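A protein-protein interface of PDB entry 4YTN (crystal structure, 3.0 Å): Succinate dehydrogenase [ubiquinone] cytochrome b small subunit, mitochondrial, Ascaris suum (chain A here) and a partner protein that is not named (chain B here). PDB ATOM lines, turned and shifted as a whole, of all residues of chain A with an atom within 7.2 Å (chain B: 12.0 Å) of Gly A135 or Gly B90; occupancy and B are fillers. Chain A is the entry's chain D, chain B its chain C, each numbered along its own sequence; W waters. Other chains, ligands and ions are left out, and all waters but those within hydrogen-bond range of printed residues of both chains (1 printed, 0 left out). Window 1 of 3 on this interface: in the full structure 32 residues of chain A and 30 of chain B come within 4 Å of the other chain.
The backbone carbonyl oxygen (O) of Gly A135 lies close to the backbone carbonyl oxygen (O) of Gly B90 (3.4 Å).
Leu B87 touches Cys A131.
Cys A131 touches Val B91.
CD1 of Leu A132 touches CB of Leu B86, 3.6 Å away.
Leu B87 touches Leu A132 (CD1 to N, 3.4 Å).
CA of Gly A135 touches N of Val B91 (3.9 Å).
Leu B86 touches Leu A136 (O to CD1, 3.8 Å).
Phe B93 touches Tyr A138 (O to CE1, 3.9 Å).
Tyr A138 touches Ser B94.
Phe A139 touches Phe B100.
No residue of chain B comes within 4 Å of Leu A133.
No residue of chain B comes within 4 Å of Ala A134.
Gly A135 touches two residues of chain B.
Of chain B, only Leu B86 (3.8 Å) comes within 4 Å of Leu A136.
Tyr A138 touches just these residues of chain B: Phe B93 (3.9 Å) and Ser B94 (3.2 Å).
Phe A139 touches just one residue of chain B: Phe B100.
Of the printed residues of chain A, Leu B86 touches Leu A132 and Leu A136.
Ile B88 touches none of the printed residues of chain A.
No residue of chain A comes within 4 Å of Gly B89.
Gly B90 touches just one residue of chain A: Gly A135 (3.3 Å).
Printed residues of chain A within 4 Å of Phe B93: Tyr A138.
The nearest residue of chain A that does not touch Gly B90 is Leu A136 (4.4 Å).
The nearest printed residue of chain A that does not touch Leu B86 is Gly A135 (5.4 Å).
The side-chain hydroxyl (OG) of Ser B94 lies within hydrogen-bond range of the backbone carbonyl oxygen (O) of Val B91 (3.0 Å).
O of Leu A136 sits close to OD1 of Asn A140, 3.5 Å away.
Printed residues of chain A that touch a printed residue of chain B: Cys A131, Leu A132, Gly A135, Leu A136, Tyr A138 and Phe A139.
Along chain A the printed residues that touch a printed residue of chain B span positions 131 to 139.
Among the printed residues, 10 pairs touch across the chains.
Among the printed residues, no Asp or Glu carboxylate lies within 4 Å of a Lys or Arg side-chain nitrogen of the other chain.
Water W1 lies within hydrogen-bond range of O of Leu B86 (2.7 Å), O of Leu A132 (2.8 Å) and N of Leu A136 (3.4 Å).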
ATOM      1  N   THR A 129      28.996  -4.340  20.579  1.00  0.00           N
ATOM      2  CA  THR A 129      30.449  -4.198  20.584  1.00  0.00           C
ATOM      3  C   THR A 129      30.972  -3.701  19.237  1.00  0.00           C
ATOM      4  O   THR A 129      31.714  -2.725  19.176  1.00  0.00           O
ATOM      5  CB  THR A 129      31.116  -5.530  20.967  1.00  0.00           C
ATOM      6  OG1 THR A 129      30.960  -5.725  22.373  1.00  0.00           O
ATOM      7  CG2 THR A 129      32.594  -5.552  20.635  1.00  0.00           C
ATOM      8  N   ALA A 130      30.570  -4.364  18.161  1.00  0.00           N
ATOM      9  CA  ALA A 130      31.080  -4.041  16.829  1.00  0.00           C
ATOM     10  C   ALA A 130      30.634  -2.666  16.327  1.00  0.00           C
ATOM     11  O   ALA A 130      31.383  -1.990  15.618  1.00  0.00           O
ATOM     12  CB  ALA A 130      30.683  -5.122  15.838  1.00  0.00           C
ATOM     13  N   CYS A 131      29.418  -2.260  16.680  1.00  0.00           N
ATOM     14  CA  CYS A 131      28.927  -0.922  16.332  1.00  0.00           C
ATOM     15  C   CYS A 131      29.552   0.157  17.222  1.00  0.00           C
ATOM     16  O   CYS A 131      29.799   1.277  16.767  1.00  0.00           O
ATOM     17  CB  CYS A 131      27.399  -0.861  16.419  1.00  0.00           C
ATOM     18  SG  CYS A 131      26.580  -2.006  15.285  1.00  0.00           S
ATOM     19  N   LEU A 132      29.804  -0.177  18.485  1.00  0.00           N
ATOM     20  CA  LEU A 132      30.479   0.742  19.385  1.00  0.00           C
ATOM     21  C   LEU A 132      31.831   1.123  18.804  1.00  0.00           C
ATOM     22  O   LEU A 132      32.152   2.300  18.698  1.00  0.00           O
ATOM     23  CB  LEU A 132      30.672   0.111  20.764  1.00  0.00           C
ATOM     24  CG  LEU A 132      31.484   0.920  21.778  1.00  0.00           C
ATOM     25  CD1 LEU A 132      30.782   2.229  22.126  1.00  0.00           C
ATOM     26  CD2 LEU A 132      31.731   0.076  23.015  1.00  0.00           C
ATOM     27  N   LEU A 133      32.620   0.124  18.425  1.00  0.00           N
ATOM     28  CA  LEU A 133      33.938   0.384  17.841  1.00  0.00           C
ATOM     29  C   LEU A 133      33.842   1.202  16.550  1.00  0.00           C
ATOM     30  O   LEU A 133      34.492   2.237  16.415  1.00  0.00           O
ATOM     31  CB  LEU A 133      34.683  -0.922  17.553  1.00  0.00           C
ATOM     32  CG  LEU A 133      36.116  -0.726  17.059  1.00  0.00           C
ATOM     33  CD1 LEU A 133      36.991  -0.181  18.176  1.00  0.00           C
ATOM     34  CD2 LEU A 133      36.689  -2.026  16.518  1.00  0.00           C
ATOM     35  N   ALA A 134      33.038   0.721  15.608  1.00  0.00           N
ATOM     36  CA  ALA A 134      32.829   1.411  14.345  1.00  0.00           C
ATOM     37  C   ALA A 134      32.541   2.898  14.579  1.00  0.00           C
ATOM     38  O   ALA A 134      33.188   3.758  13.983  1.00  0.00           O
ATOM     39  CB  ALA A 134      31.694   0.753  13.576  1.00  0.00           C
ATOM     40  N   GLY A 135      31.593   3.187  15.469  1.00  0.00           N
ATOM     41  CA  GLY A 135      31.223   4.565  15.807  1.00  0.00           C
ATOM     42  C   GLY A 135      32.300   5.368  16.527  1.00  0.00           C
ATOM     43  O   GLY A 135      32.351   6.589  16.402  1.00  0.00           O
ATOM     44  N   LEU A 136      33.154   4.692  17.293  1.00  0.00           N
ATOM     45  CA  LEU A 136      34.293   5.344  17.953  1.00  0.00           C
ATOM     46  C   LEU A 136      35.419   5.670  16.961  1.00  0.00           C
ATOM     47  O   LEU A 136      35.937   6.790  16.955  1.00  0.00           O
ATOM     48  CB  LEU A 136      34.829   4.475  19.105  1.00  0.00           C
ATOM     49  CG  LEU A 136      34.612   4.928  20.557  1.00  0.00           C
ATOM     50  CD1 LEU A 136      33.412   5.841  20.771  1.00  0.00           C
ATOM     51  CD2 LEU A 136      34.518   3.699  21.452  1.00  0.00           C
ATOM     52  N   LEU A 137      35.797   4.691  16.138  1.00  0.00           N
ATOM     53  CA  LEU A 137      36.826   4.882  15.103  1.00  0.00           C
ATOM     54  C   LEU A 137      36.433   6.012  14.160  1.00  0.00           C
ATOM     55  O   LEU A 137      37.271   6.838  13.783  1.00  0.00           O
ATOM     56  CB  LEU A 137      37.021   3.607  14.277  1.00  0.00           C
ATOM     57  CG  LEU A 137      37.616   2.387  14.964  1.00  0.00           C
ATOM     58  CD1 LEU A 137      37.571   1.196  14.022  1.00  0.00           C
ATOM     59  CD2 LEU A 137      39.036   2.668  15.413  1.00  0.00           C
ATOM     60  N   TYR A 138      35.158   6.029  13.769  1.00  0.00           N
ATOM     61  CA  TYR A 138      34.638   7.094  12.934  1.00  0.00           C
ATOM     62  C   TYR A 138      34.838   8.443  13.607  1.00  0.00           C
ATOM     63  O   TYR A 138      35.358   9.371  12.996  1.00  0.00           O
ATOM     64  CB  TYR A 138      33.152   6.901  12.645  1.00  0.00           C
ATOM     65  CG  TYR A 138      32.581   8.105  11.953  1.00  0.00           C
ATOM     66  CD1 TYR A 138      32.026   9.158  12.686  1.00  0.00           C
ATOM     67  CD2 TYR A 138      32.655   8.229  10.565  1.00  0.00           C
ATOM     68  CE1 TYR A 138      31.534  10.286  12.052  1.00  0.00           C
ATOM     69  CE2 TYR A 138      32.167   9.355   9.919  1.00  0.00           C
ATOM     70  CZ  TYR A 138      31.605  10.378  10.667  1.00  0.00           C
ATOM     71  OH  TYR A 138      31.108  11.492  10.033  1.00  0.00           O
ATOM     72  N   PHE A 139      34.415   8.548  14.864  1.00  0.00           N
ATOM     73  CA  PHE A 139      34.509   9.801  15.621  1.00  0.00           C
ATOM     74  C   PHE A 139      35.956  10.269  15.811  1.00  0.00           C
ATOM     75  O   PHE A 139      36.219  11.471  15.886  1.00  0.00           O
ATOM     76  CB  PHE A 139      33.846   9.633  16.986  1.00  0.00           C
ATOM     77  CG  PHE A 139      33.619  10.924  17.724  1.00  0.00           C
ATOM     78  CD1 PHE A 139      32.441  11.635  17.550  1.00  0.00           C
ATOM     79  CD2 PHE A 139      34.566  11.409  18.612  1.00  0.00           C
ATOM     80  CE1 PHE A 139      32.212  12.810  18.242  1.00  0.00           C
ATOM     81  CE2 PHE A 139      34.344  12.585  19.305  1.00  0.00           C
ATOM     82  CZ  PHE A 139      33.166  13.285  19.123  1.00  0.00           C
ATOM     83  N   ASN A 140      36.883   9.319  15.915  1.00  0.00           N
ATOM     84  CA  ASN A 140      38.305   9.644  15.984  1.00  0.00           C
ATOM     85  C   ASN A 140      38.767  10.186  14.644  1.00  0.00           C
ATOM     86  O   ASN A 140      39.269  11.307  14.546  1.00  0.00           O
ATOM     87  CB  ASN A 140      39.143   8.403  16.341  1.00  0.00           C
ATOM     88  CG  ASN A 140      38.902   7.894  17.758  1.00  0.00           C
ATOM     89  OD1 ASN A 140      39.218   6.739  18.061  1.00  0.00           O
ATOM     90  ND2 ASN A 140      38.365   8.749  18.635  1.00  0.00           N
ATOM     91  N   CYS B  80      27.075   1.152  32.271  1.00  0.00           N
ATOM     92  CA  CYS B  80      26.149   1.055  31.132  1.00  0.00           C
ATOM     93  C   CYS B  80      25.853   2.405  30.475  1.00  0.00           C
ATOM     94  O   CYS B  80      25.818   2.495  29.245  1.00  0.00           O
ATOM     95  CB  CYS B  80      24.836   0.390  31.559  1.00  0.00           C
ATOM     96  SG  CYS B  80      25.011  -1.389  31.818  1.00  0.00           S
ATOM     97  N   ALA B  81      25.627   3.444  31.282  1.00  0.00           N
ATOM     98  CA  ALA B  81      25.365   4.783  30.747  1.00  0.00           C
ATOM     99  C   ALA B  81      26.587   5.298  29.972  1.00  0.00           C
ATOM    100  O   ALA B  81      26.444   5.924  28.917  1.00  0.00           O
ATOM    101  CB  ALA B  81      24.979   5.748  31.859  1.00  0.00           C
ATOM    102  N   MET B  82      27.784   5.013  30.485  1.00  0.00           N
ATOM    103  CA  MET B  82      29.017   5.382  29.784  1.00  0.00           C
ATOM    104  C   MET B  82      29.146   4.588  28.479  1.00  0.00           C
ATOM    105  O   MET B  82      29.516   5.153  27.452  1.00  0.00           O
ATOM    106  CB  MET B  82      30.261   5.189  30.667  1.00  0.00           C
ATOM    107  CG  MET B  82      30.287   6.058  31.924  1.00  0.00           C
ATOM    108  SD  MET B  82      31.873   6.060  32.806  1.00  0.00           S
ATOM    109  CE  MET B  82      32.163   4.318  33.117  1.00  0.00           C
ATOM    110  N   ALA B  83      28.827   3.297  28.497  1.00  0.00           N
ATOM    111  CA  ALA B  83      28.795   2.542  27.248  1.00  0.00           C
ATOM    112  C   ALA B  83      27.788   3.203  26.314  1.00  0.00           C
ATOM    113  O   ALA B  83      28.141   3.659  25.223  1.00  0.00           O
ATOM    114  CB  ALA B  83      28.425   1.087  27.485  1.00  0.00           C
ATOM    115  N   GLY B  84      26.543   3.283  26.774  1.00  0.00           N
ATOM    116  CA  GLY B  84      25.448   3.833  25.985  1.00  0.00           C
ATOM    117  C   GLY B  84      25.804   5.133  25.310  1.00  0.00           C
ATOM    118  O   GLY B  84      25.568   5.303  24.115  1.00  0.00           O
ATOM    119  N   THR B  85      26.393   6.046  26.075  1.00  0.00           N
ATOM    120  CA  THR B  85      26.785   7.350  25.543  1.00  0.00           C
ATOM    121  C   THR B  85      27.800   7.208  24.415  1.00  0.00           C
ATOM    122  O   THR B  85      27.592   7.759  23.334  1.00  0.00           O
ATOM    123  CB  THR B  85      27.340   8.258  26.643  1.00  0.00           C
ATOM    124  OG1 THR B  85      26.327   8.448  27.630  1.00  0.00           O
ATOM    125  CG2 THR B  85      27.720   9.602  26.087  1.00  0.00           C
ATOM    126  N   LEU B  86      28.871   6.452  24.660  1.00  0.00           N
ATOM    127  CA  LEU B  86      29.865   6.164  23.622  1.00  0.00           C
ATOM    128  C   LEU B  86      29.265   5.543  22.362  1.00  0.00           C
ATOM    129  O   LEU B  86      29.671   5.915  21.269  1.00  0.00           O
ATOM    130  CB  LEU B  86      30.973   5.246  24.143  1.00  0.00           C
ATOM    131  CG  LEU B  86      31.955   5.795  25.180  1.00  0.00           C
ATOM    132  CD1 LEU B  86      33.104   4.809  25.342  1.00  0.00           C
ATOM    133  CD2 LEU B  86      32.479   7.170  24.805  1.00  0.00           C
ATOM    134  N   LEU B  87      28.318   4.612  22.498  1.00  0.00           N
ATOM    135  CA  LEU B  87      27.658   4.024  21.317  1.00  0.00           C
ATOM    136  C   LEU B  87      26.708   5.006  20.635  1.00  0.00           C
ATOM    137  O   LEU B  87      26.803   5.204  19.426  1.00  0.00           O
ATOM    138  CB  LEU B  87      26.886   2.751  21.651  1.00  0.00           C
ATOM    139  CG  LEU B  87      26.082   2.184  20.464  1.00  0.00           C
ATOM    140  CD1 LEU B  87      26.993   1.512  19.443  1.00  0.00           C
ATOM    141  CD2 LEU B  87      25.005   1.214  20.928  1.00  0.00           C
ATOM    142  N   ILE B  88      25.781   5.597  21.389  1.00  0.00           N
ATOM    143  CA  ILE B  88      24.873   6.590  20.802  1.00  0.00           C
ATOM    144  C   ILE B  88      25.712   7.720  20.213  1.00  0.00           C
ATOM    145  O   ILE B  88      25.542   8.083  19.058  1.00  0.00           O
ATOM    146  CB  ILE B  88      23.863   7.192  21.813  1.00  0.00           C
ATOM    147  CG1 ILE B  88      22.970   6.106  22.447  1.00  0.00           C
ATOM    148  CG2 ILE B  88      23.011   8.263  21.139  1.00  0.00           C
ATOM    149  CD1 ILE B  88      21.984   5.447  21.506  1.00  0.00           C
ATOM    150  N   GLY B  89      26.628   8.256  21.012  1.00  0.00           N
ATOM    151  CA  GLY B  89      27.507   9.335  20.571  1.00  0.00           C
ATOM    152  C   GLY B  89      28.300   8.958  19.341  1.00  0.00           C
ATOM    153  O   GLY B  89      28.287   9.671  18.346  1.00  0.00           O
ATOM    154  N   GLY B  90      28.985   7.822  19.402  1.00  0.00           N
ATOM    155  CA  GLY B  90      29.821   7.379  18.294  1.00  0.00           C
ATOM    156  C   GLY B  90      29.016   7.219  17.018  1.00  0.00           C
ATOM    157  O   GLY B  90      29.261   7.911  16.029  1.00  0.00           O
ATOM    158  N   VAL B  91      28.034   6.324  17.057  1.00  0.00           N
ATOM    159  CA  VAL B  91      27.203   6.023  15.887  1.00  0.00           C
ATOM    160  C   VAL B  91      26.280   7.188  15.497  1.00  0.00           C
ATOM    161  O   VAL B  91      25.960   7.359  14.324  1.00  0.00           O
ATOM    162  CB  VAL B  91      26.380   4.736  16.115  1.00  0.00           C
ATOM    163  CG1 VAL B  91      25.384   4.502  14.986  1.00  0.00           C
ATOM    164  CG2 VAL B  91      27.317   3.541  16.271  1.00  0.00           C
ATOM    165  N   GLY B  92      25.870   7.991  16.473  1.00  0.00           N
ATOM    166  CA  GLY B  92      24.970   9.115  16.217  1.00  0.00           C
ATOM    167  C   GLY B  92      25.585  10.184  15.338  1.00  0.00           C
ATOM    168  O   GLY B  92      25.017  10.547  14.313  1.00  0.00           O
ATOM    169  N   PHE B  93      26.757  10.678  15.729  1.00  0.00           N
ATOM    170  CA  PHE B  93      27.403  11.776  15.007  1.00  0.00           C
ATOM    171  C   PHE B  93      27.938  11.354  13.636  1.00  0.00           C
ATOM    172  O   PHE B  93      28.267  12.210  12.810  1.00  0.00           O
ATOM    173  CB  PHE B  93      28.513  12.409  15.854  1.00  0.00           C
ATOM    174  CG  PHE B  93      28.002  13.333  16.927  1.00  0.00           C
ATOM    175  CD1 PHE B  93      27.570  12.835  18.147  1.00  0.00           C
ATOM    176  CD2 PHE B  93      27.944  14.706  16.713  1.00  0.00           C
ATOM    177  CE1 PHE B  93      27.092  13.684  19.134  1.00  0.00           C
ATOM    178  CE2 PHE B  93      27.466  15.560  17.698  1.00  0.00           C
ATOM    179  CZ  PHE B  93      27.039  15.048  18.909  1.00  0.00           C
ATOM    180  N   SER B  94      28.015  10.044  13.398  1.00  0.00           N
ATOM    181  CA  SER B  94      28.385   9.506  12.086  1.00  0.00           C
ATOM    182  C   SER B  94      27.169   9.373  11.173  1.00  0.00           C
ATOM    183  O   SER B  94      27.216   9.750  10.003  1.00  0.00           O
ATOM    184  CB  SER B  94      29.058   8.138  12.236  1.00  0.00           C
ATOM    185  OG  SER B  94      28.097   7.104  12.264  1.00  0.00           O
ATOM    186  N   VAL B  95      26.086   8.828  11.712  1.00  0.00           N
ATOM    187  CA  VAL B  95      24.857   8.620  10.948  1.00  0.00           C
ATOM    188  C   VAL B  95      24.109   9.938  10.687  1.00  0.00           C
ATOM    189  O   VAL B  95      23.317  10.020   9.753  1.00  0.00           O
ATOM    190  CB  VAL B  95      23.951   7.572  11.647  1.00  0.00           C
ATOM    191  CG1 VAL B  95      22.545   7.543  11.057  1.00  0.00           C
ATOM    192  CG2 VAL B  95      24.594   6.191  11.555  1.00  0.00           C
ATOM    193  N   LEU B  96      24.368  10.965  11.493  1.00  0.00           N
ATOM    194  CA  LEU B  96      23.780  12.292  11.261  1.00  0.00           C
ATOM    195  C   LEU B  96      24.764  13.193  10.494  1.00  0.00           C
ATOM    196  O   LEU B  96      25.984  12.991  10.568  1.00  0.00           O
ATOM    197  CB  LEU B  96      23.374  12.953  12.590  1.00  0.00           C
ATOM    198  CG  LEU B  96      22.022  12.585  13.222  1.00  0.00           C
ATOM    199  CD1 LEU B  96      21.790  11.084  13.238  1.00  0.00           C
ATOM    200  CD2 LEU B  96      21.924  13.148  14.633  1.00  0.00           C
ATOM    201  N   PRO B  97      24.237  14.199   9.762  1.00  0.00           N
ATOM    202  CA  PRO B  97      25.085  15.161   9.050  1.00  0.00           C
ATOM    203  C   PRO B  97      25.758  16.152   9.998  1.00  0.00           C
ATOM    204  O   PRO B  97      26.717  16.818   9.617  1.00  0.00           O
ATOM    205  CB  PRO B  97      24.094  15.891   8.146  1.00  0.00           C
ATOM    206  CG  PRO B  97      22.815  15.858   8.911  1.00  0.00           C
ATOM    207  CD  PRO B  97      22.804  14.537   9.626  1.00  0.00           C
ATOM    208  N   LEU B  98      25.230  16.251  11.215  1.00  0.00           N
ATOM    209  CA  LEU B  98      25.814  17.058  12.280  1.00  0.00           C
ATOM    210  C   LEU B  98      27.215  16.558  12.683  1.00  0.00           C
ATOM    211  O   LEU B  98      27.493  15.353  12.635  1.00  0.00           O
ATOM    212  CB  LEU B  98      24.872  17.029  13.493  1.00  0.00           C
ATOM    213  CG  LEU B  98      25.239  17.820  14.749  1.00  0.00           C
ATOM    214  CD1 LEU B  98      25.146  19.313  14.493  1.00  0.00           C
ATOM    215  CD2 LEU B  98      24.336  17.429  15.908  1.00  0.00           C
ATOM    216  N   ASP B  99      28.088  17.496  13.058  1.00  0.00           N
ATOM    217  CA  ASP B  99      29.405  17.178  13.625  1.00  0.00           C
ATOM    218  C   ASP B  99      29.468  17.652  15.076  1.00  0.00           C
ATOM    219  O   ASP B  99      28.561  18.332  15.556  1.00  0.00           O
ATOM    220  CB  ASP B  99      30.554  17.787  12.787  1.00  0.00           C
ATOM    221  CG  ASP B  99      30.592  19.321  12.827  1.00  0.00           C
ATOM    222  OD1 ASP B  99      29.640  19.948  13.329  1.00  0.00           O
ATOM    223  OD2 ASP B  99      31.583  19.905  12.340  1.00  0.00           O
ATOM    224  N   PHE B 100      30.542  17.298  15.770  1.00  0.00           N
ATOM    225  CA  PHE B 100      30.657  17.625  17.190  1.00  0.00           C
ATOM    226  C   PHE B 100      30.789  19.132  17.426  1.00  0.00           C
ATOM    227  O   PHE B 100      30.229  19.662  18.384  1.00  0.00           O
ATOM    228  CB  PHE B 100      31.834  16.874  17.835  1.00  0.00           C
ATOM    229  CG  PHE B 100      31.751  16.793  19.337  1.00  0.00           C
ATOM    230  CD1 PHE B 100      32.580  17.562  20.138  1.00  0.00           C
ATOM    231  CD2 PHE B 100      30.833  15.952  19.951  1.00  0.00           C
ATOM    232  CE1 PHE B 100      32.500  17.489  21.521  1.00  0.00           C
ATOM    233  CE2 PHE B 100      30.748  15.880  21.332  1.00  0.00           C
ATOM    234  CZ  PHE B 100      31.582  16.648  22.117  1.00  0.00           C
ATOM    235  N   PHE B 103      27.558  20.969  17.411  1.00  0.00           N
ATOM    236  CA  PHE B 103      26.822  20.549  18.609  1.00  0.00           C
ATOM    237  C   PHE B 103      27.292  21.320  19.850  1.00  0.00           C
ATOM    238  O   PHE B 103      26.466  21.792  20.632  1.00  0.00           O
ATOM    239  CB  PHE B 103      26.944  19.034  18.819  1.00  0.00           C
ATOM    240  CG  PHE B 103      26.411  18.551  20.146  1.00  0.00           C
ATOM    241  CD1 PHE B 103      25.069  18.716  20.471  1.00  0.00           C
ATOM    242  CD2 PHE B 103      27.248  17.916  21.061  1.00  0.00           C
ATOM    243  CE1 PHE B 103      24.574  18.267  21.686  1.00  0.00           C
ATOM    244  CE2 PHE B 103      26.758  17.466  22.275  1.00  0.00           C
ATOM    245  CZ  PHE B 103      25.418  17.641  22.588  1.00  0.00           C
HETATM  246  O   HOH W   1      30.363   4.340  19.155  1.00  0.00           O
